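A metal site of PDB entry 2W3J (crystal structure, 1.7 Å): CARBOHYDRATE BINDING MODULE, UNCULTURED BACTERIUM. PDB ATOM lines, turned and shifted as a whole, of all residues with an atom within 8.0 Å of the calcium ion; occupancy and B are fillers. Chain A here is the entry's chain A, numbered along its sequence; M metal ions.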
ATOM      1  N   LEU A   3      -4.562 -31.623  18.511  1.00  0.00           N
ATOM      2  CA  LEU A   3      -4.854 -30.192  18.484  1.00  0.00           C
ATOM      3  C   LEU A   3      -4.137 -29.524  19.631  1.00  0.00           C
ATOM      4  O   LEU A   3      -4.392 -29.842  20.811  1.00  0.00           O
ATOM      5  CB  LEU A   3      -6.370 -29.997  18.601  1.00  0.00           C
ATOM      6  CG  LEU A   3      -6.866 -28.546  18.677  1.00  0.00           C
ATOM      7  CD1 LEU A   3      -6.503 -27.804  17.398  1.00  0.00           C
ATOM      8  CD2 LEU A   3      -8.423 -28.498  18.921  1.00  0.00           C
ATOM      9  N   PHE A   4      -3.242 -28.593  19.306  1.00  0.00           N
ATOM     10  CA  PHE A   4      -2.363 -27.951  20.290  1.00  0.00           C
ATOM     11  C   PHE A   4      -2.918 -26.555  20.670  1.00  0.00           C
ATOM     12  O   PHE A   4      -3.017 -25.705  19.819  1.00  0.00           O
ATOM     13  CB  PHE A   4      -0.960 -27.727  19.694  1.00  0.00           C
ATOM     14  CG  PHE A   4      -0.199 -29.025  19.447  1.00  0.00           C
ATOM     15  CD1 PHE A   4       0.757 -29.432  20.353  1.00  0.00           C
ATOM     16  CD2 PHE A   4      -0.457 -29.796  18.318  1.00  0.00           C
ATOM     17  CE1 PHE A   4       1.482 -30.633  20.142  1.00  0.00           C
ATOM     18  CE2 PHE A   4       0.235 -31.004  18.117  1.00  0.00           C
ATOM     19  CZ  PHE A   4       1.194 -31.398  19.034  1.00  0.00           C
ATOM     20  N   GLU A   5      -3.241 -26.389  21.941  1.00  0.00           N
ATOM     21  CA  GLU A   5      -3.773 -25.140  22.500  1.00  0.00           C
ATOM     22  C   GLU A   5      -2.697 -24.489  23.363  1.00  0.00           C
ATOM     23  O   GLU A   5      -1.833 -25.157  23.977  1.00  0.00           O
ATOM     24  CB  GLU A   5      -4.986 -25.455  23.377  1.00  0.00           C
ATOM     25  CG  GLU A   5      -6.110 -26.096  22.593  1.00  0.00           C
ATOM     26  CD  GLU A   5      -6.893 -25.099  21.750  1.00  0.00           C
ATOM     27  OE1 GLU A   5      -6.634 -23.879  21.843  1.00  0.00           O
ATOM     28  OE2 GLU A   5      -7.797 -25.544  20.991  1.00  0.00           O
ATOM     29  N   GLU A   6      -2.778 -23.165  23.482  1.00  0.00           N
ATOM     30  CA  GLU A   6      -1.926 -22.480  24.435  1.00  0.00           C
ATOM     31  C   GLU A   6      -2.172 -22.983  25.861  1.00  0.00           C
ATOM     32  O   GLU A   6      -3.286 -23.411  26.213  1.00  0.00           O
ATOM     33  CB  GLU A   6      -2.153 -20.980  24.324  1.00  0.00           C
ATOM     34  CG  GLU A   6      -3.508 -20.470  24.808  1.00  0.00           C
ATOM     35  CD  GLU A   6      -4.720 -21.028  24.036  1.00  0.00           C
ATOM     36  OE1 GLU A   6      -4.626 -21.264  22.811  1.00  0.00           O
ATOM     37  OE2 GLU A   6      -5.795 -21.203  24.678  1.00  0.00           O
ATOM     38  N   SER A   7      -1.101 -22.981  26.644  1.00  0.00           N
ATOM     39  CA  SER A   7      -1.125 -23.415  28.048  1.00  0.00           C
ATOM     40  C   SER A   7      -1.504 -24.902  28.232  1.00  0.00           C
ATOM     41  O   SER A   7      -1.906 -25.319  29.322  1.00  0.00           O
ATOM     42  CB  SER A   7      -2.062 -22.511  28.875  1.00  0.00           C
ATOM     43  OG  SER A   7      -1.784 -21.143  28.627  1.00  0.00           O
ATOM     44  N   ILE A  18      -1.230 -14.162  26.370  1.00  0.00           N
ATOM     45  CA  ILE A  18      -2.346 -14.996  26.044  1.00  0.00           C
ATOM     46  C   ILE A  18      -3.571 -14.129  26.356  1.00  0.00           C
ATOM     47  O   ILE A  18      -3.582 -13.388  27.355  1.00  0.00           O
ATOM     48  CB  ILE A  18      -2.320 -16.273  26.899  1.00  0.00           C
ATOM     49  CG1 ILE A  18      -1.059 -17.102  26.544  1.00  0.00           C
ATOM     50  CG2 ILE A  18      -3.625 -17.084  26.787  1.00  0.00           C
ATOM     51  CD1 ILE A  18      -0.788 -18.213  27.498  1.00  0.00           C
ATOM     52  N   ASP A  19      -4.590 -14.235  25.520  1.00  0.00           N
ATOM     53  CA  ASP A  19      -5.774 -13.384  25.711  1.00  0.00           C
ATOM     54  C   ASP A  19      -7.025 -14.096  25.245  1.00  0.00           C
ATOM     55  O   ASP A  19      -6.956 -15.170  24.661  1.00  0.00           O
ATOM     56  CB  ASP A  19      -5.618 -12.052  24.996  1.00  0.00           C
ATOM     57  CG  ASP A  19      -6.528 -10.948  25.597  1.00  0.00           C
ATOM     58  OD1 ASP A  19      -7.484 -11.232  26.375  1.00  0.00           O
ATOM     59  OD2 ASP A  19      -6.284  -9.798  25.249  1.00  0.00           O
ATOM     60  N   GLY A  24     -14.728 -16.838  20.147  1.00  0.00           N
ATOM     61  CA  GLY A  24     -14.668 -17.779  19.030  1.00  0.00           C
ATOM     62  C   GLY A  24     -13.438 -18.657  19.035  1.00  0.00           C
ATOM     63  O   GLY A  24     -13.335 -19.573  18.200  1.00  0.00           O
ATOM     64  N   TYR A  25     -12.518 -18.387  19.952  1.00  0.00           N
ATOM     65  CA  TYR A  25     -11.333 -19.237  20.110  1.00  0.00           C
ATOM     66  C   TYR A  25     -11.719 -20.625  20.670  1.00  0.00           C
ATOM     67  O   TYR A  25     -12.851 -20.851  21.140  1.00  0.00           O
ATOM     68  CB  TYR A  25     -10.304 -18.575  21.054  1.00  0.00           C
ATOM     69  CG  TYR A  25     -10.960 -18.171  22.361  1.00  0.00           C
ATOM     70  CD1 TYR A  25     -11.143 -19.112  23.404  1.00  0.00           C
ATOM     71  CD2 TYR A  25     -11.414 -16.879  22.545  1.00  0.00           C
ATOM     72  CE1 TYR A  25     -11.771 -18.730  24.574  1.00  0.00           C
ATOM     73  CE2 TYR A  25     -12.048 -16.504  23.717  1.00  0.00           C
ATOM     74  CZ  TYR A  25     -12.228 -17.422  24.706  1.00  0.00           C
ATOM     75  OH  TYR A  25     -12.863 -16.997  25.859  1.00  0.00           O
ATOM     76  N   THR A  26     -10.771 -21.550  20.632  1.00  0.00           N
ATOM     77  CA  THR A  26     -10.922 -22.817  21.304  1.00  0.00           C
ATOM     78  C   THR A  26      -9.932 -22.865  22.474  1.00  0.00           C
ATOM     79  O   THR A  26      -9.052 -22.015  22.596  1.00  0.00           O
ATOM     80  CB  THR A  26     -10.668 -23.994  20.357  1.00  0.00           C
ATOM     81  OG1 THR A  26      -9.356 -23.880  19.811  1.00  0.00           O
ATOM     82  CG2 THR A  26     -11.700 -24.004  19.232  1.00  0.00           C
ATOM     83  N   GLY A  27     -10.098 -23.816  23.394  1.00  0.00           N
ATOM     84  CA  GLY A  27      -9.280 -23.799  24.593  1.00  0.00           C
ATOM     85  C   GLY A  27      -9.574 -22.554  25.408  1.00  0.00           C
ATOM     86  O   GLY A  27     -10.725 -22.071  25.418  1.00  0.00           O
ATOM     87  N   THR A  28      -8.567 -22.032  26.080  1.00  0.00           N
ATOM     88  CA  THR A  28      -8.720 -20.895  27.012  1.00  0.00           C
ATOM     89  C   THR A  28      -8.648 -19.537  26.317  1.00  0.00           C
ATOM     90  O   THR A  28      -8.973 -18.490  26.915  1.00  0.00           O
ATOM     91  CB  THR A  28      -7.587 -20.895  28.124  1.00  0.00           C
ATOM     92  OG1 THR A  28      -6.300 -20.576  27.550  1.00  0.00           O
ATOM     93  CG2 THR A  28      -7.490 -22.200  28.815  1.00  0.00           C
ATOM     94  N   GLY A  29      -8.156 -19.502  25.079  1.00  0.00           N
ATOM     95  CA  GLY A  29      -7.858 -18.193  24.494  1.00  0.00           C
ATOM     96  C   GLY A  29      -6.965 -18.355  23.291  1.00  0.00           C
ATOM     97  O   GLY A  29      -7.074 -19.344  22.592  1.00  0.00           O
ATOM     98  N   PHE A  30      -6.091 -17.400  23.080  1.00  0.00           N
ATOM     99  CA  PHE A  30      -5.231 -17.444  21.902  1.00  0.00           C
ATOM    100  C   PHE A  30      -4.002 -16.628  22.230  1.00  0.00           C
ATOM    101  O   PHE A  30      -3.978 -15.922  23.259  1.00  0.00           O
ATOM    102  CB  PHE A  30      -5.940 -16.807  20.694  1.00  0.00           C
ATOM    103  CG  PHE A  30      -6.562 -15.459  20.980  1.00  0.00           C
ATOM    104  CD1 PHE A  30      -5.814 -14.284  20.861  1.00  0.00           C
ATOM    105  CD2 PHE A  30      -7.898 -15.368  21.350  1.00  0.00           C
ATOM    106  CE1 PHE A  30      -6.375 -13.025  21.123  1.00  0.00           C
ATOM    107  CE2 PHE A  30      -8.478 -14.087  21.577  1.00  0.00           C
ATOM    108  CZ  PHE A  30      -7.703 -12.933  21.469  1.00  0.00           C
ATOM    109  N   ILE A  31      -2.986 -16.723  21.368  1.00  0.00           N
ATOM    110  CA  ILE A  31      -1.775 -15.923  21.533  1.00  0.00           C
ATOM    111  C   ILE A  31      -1.903 -14.569  20.822  1.00  0.00           C
ATOM    112  O   ILE A  31      -2.263 -14.500  19.678  1.00  0.00           O
ATOM    113  CB  ILE A  31      -0.547 -16.659  20.960  1.00  0.00           C
ATOM    114  CG1 ILE A  31      -0.359 -18.012  21.671  1.00  0.00           C
ATOM    115  CG2 ILE A  31       0.700 -15.786  21.061  1.00  0.00           C
ATOM    116  CD1 ILE A  31      -0.351 -17.961  23.194  1.00  0.00           C
ATOM    117  N   ARG A  58      -5.161 -22.155  13.147  1.00  0.00           N
ATOM    118  CA  ARG A  58      -6.396 -21.370  13.184  1.00  0.00           C
ATOM    119  C   ARG A  58      -6.047 -20.012  13.812  1.00  0.00           C
ATOM    120  O   ARG A  58      -5.350 -19.941  14.821  1.00  0.00           O
ATOM    121  CB  ARG A  58      -7.457 -22.076  14.028  1.00  0.00           C
ATOM    122  CG  ARG A  58      -8.825 -21.426  13.991  1.00  0.00           C
ATOM    123  CD  ARG A  58      -9.879 -22.346  14.679  1.00  0.00           C
ATOM    124  NE  ARG A  58     -11.247 -21.826  14.522  1.00  0.00           N
ATOM    125  CZ  ARG A  58     -11.915 -21.168  15.471  1.00  0.00           C
ATOM    126  NH1 ARG A  58     -11.360 -20.880  16.653  1.00  0.00           N
ATOM    127  NH2 ARG A  58     -13.153 -20.740  15.203  1.00  0.00           N
ATOM    128  N   TRP A  92     -12.851 -16.374  12.492  1.00  0.00           N
ATOM    129  CA  TRP A  92     -11.538 -16.971  12.592  1.00  0.00           C
ATOM    130  C   TRP A  92     -11.220 -17.622  11.235  1.00  0.00           C
ATOM    131  O   TRP A  92     -12.137 -17.961  10.474  1.00  0.00           O
ATOM    132  CB  TRP A  92     -11.527 -17.989  13.734  1.00  0.00           C
ATOM    133  CG  TRP A  92     -11.648 -17.326  15.076  1.00  0.00           C
ATOM    134  CD1 TRP A  92     -12.784 -16.842  15.674  1.00  0.00           C
ATOM    135  CD2 TRP A  92     -10.565 -17.008  15.949  1.00  0.00           C
ATOM    136  NE1 TRP A  92     -12.472 -16.271  16.895  1.00  0.00           N
ATOM    137  CE2 TRP A  92     -11.111 -16.353  17.078  1.00  0.00           C
ATOM    138  CE3 TRP A  92      -9.179 -17.236  15.886  1.00  0.00           C
ATOM    139  CZ2 TRP A  92     -10.319 -15.914  18.139  1.00  0.00           C
ATOM    140  CZ3 TRP A  92      -8.397 -16.775  16.941  1.00  0.00           C
ATOM    141  CH2 TRP A  92      -8.973 -16.150  18.069  1.00  0.00           C
ATOM    142  N   ILE A 121      -3.109 -16.294  17.326  1.00  0.00           N
ATOM    143  CA  ILE A 121      -3.058 -17.739  16.981  1.00  0.00           C
ATOM    144  C   ILE A 121      -3.860 -18.558  17.998  1.00  0.00           C
ATOM    145  O   ILE A 121      -3.525 -18.580  19.183  1.00  0.00           O
ATOM    146  CB  ILE A 121      -1.622 -18.250  16.946  1.00  0.00           C
ATOM    147  CG1 ILE A 121      -0.767 -17.389  15.997  1.00  0.00           C
ATOM    148  CG2 ILE A 121      -1.632 -19.778  16.545  1.00  0.00           C
ATOM    149  CD1 ILE A 121      -1.317 -17.370  14.558  1.00  0.00           C
ATOM    150  N   ASP A 122      -4.944 -19.160  17.530  1.00  0.00           N
ATOM    151  CA  ASP A 122      -5.850 -19.928  18.404  1.00  0.00           C
ATOM    152  C   ASP A 122      -5.255 -21.305  18.708  1.00  0.00           C
ATOM    153  O   ASP A 122      -5.286 -21.780  19.849  1.00  0.00           O
ATOM    154  CB  ASP A 122      -7.191 -20.095  17.688  1.00  0.00           C
ATOM    155  CG  ASP A 122      -8.170 -20.897  18.501  1.00  0.00           C
ATOM    156  OD1 ASP A 122      -8.156 -20.737  19.750  1.00  0.00           O
ATOM    157  OD2 ASP A 122      -8.945 -21.641  17.870  1.00  0.00           O
ATOM    158  N   SER A 123      -4.749 -21.950  17.679  1.00  0.00           N
ATOM    159  CA  SER A 123      -4.283 -23.333  17.848  1.00  0.00           C
ATOM    160  C   SER A 123      -3.527 -23.766  16.610  1.00  0.00           C
ATOM    161  O   SER A 123      -3.619 -23.148  15.538  1.00  0.00           O
ATOM    162  CB  SER A 123      -5.513 -24.258  18.004  1.00  0.00           C
ATOM    163  OG  SER A 123      -6.367 -24.164  16.841  1.00  0.00           O
ATOM    164  N   ILE A 124      -2.797 -24.859  16.750  1.00  0.00           N
ATOM    165  CA  ILE A 124      -2.282 -25.576  15.588  1.00  0.00           C
ATOM    166  C   ILE A 124      -2.726 -27.048  15.710  1.00  0.00           C
ATOM    167  O   ILE A 124      -2.689 -27.611  16.803  1.00  0.00           O
ATOM    168  CB  ILE A 124      -0.750 -25.413  15.380  1.00  0.00           C
ATOM    169  CG1 ILE A 124      -0.353 -26.021  14.039  1.00  0.00           C
ATOM    170  CG2 ILE A 124       0.125 -25.987  16.511  1.00  0.00           C
ATOM    171  CD1 ILE A 124       1.104 -25.750  13.733  1.00  0.00           C
HETATM  172 CA    CA M   1      -6.905 -21.520  21.624  1.00  0.00          CA
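The side-chain hydroxyl (OG1) of Thr 28 sits at hydrogen-bond distance from the side-chain carboxylate (OE2) of Glu 6 (3.0 Å).
The side-chain carboxylate (OD2) of Asp 122 lies within salt-bridge range of the guanidinium group (NH1) of Arg 58.
Within 4 Å of the calcium ion: Glu 5, Glu 6, Thr 26, Gly 29 and Asp 122.
Along chain A the residues within 4 Å of the calcium ion span positions 5 to 122.
The nearest printed residue that does not touch the calcium ion is Gly 27 (4.3 Å).
OE1 of Glu 5 binds the calcium ion, at 2.4 Å.
OD1 of Asp 122 binds the calcium ion.
The calcium ion is bound by the backbone carbonyl oxygen (O) of Gly 29 (2.4 Å).
The backbone carbonyl oxygen (O) of Thr 26 binds the calcium ion.
The calcium ion is bound by the backbone carbonyl oxygen (O) of Asp 122 (2.4 Å).
OE1 of Glu 6 is bound to the calcium ion (2.6 Å).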
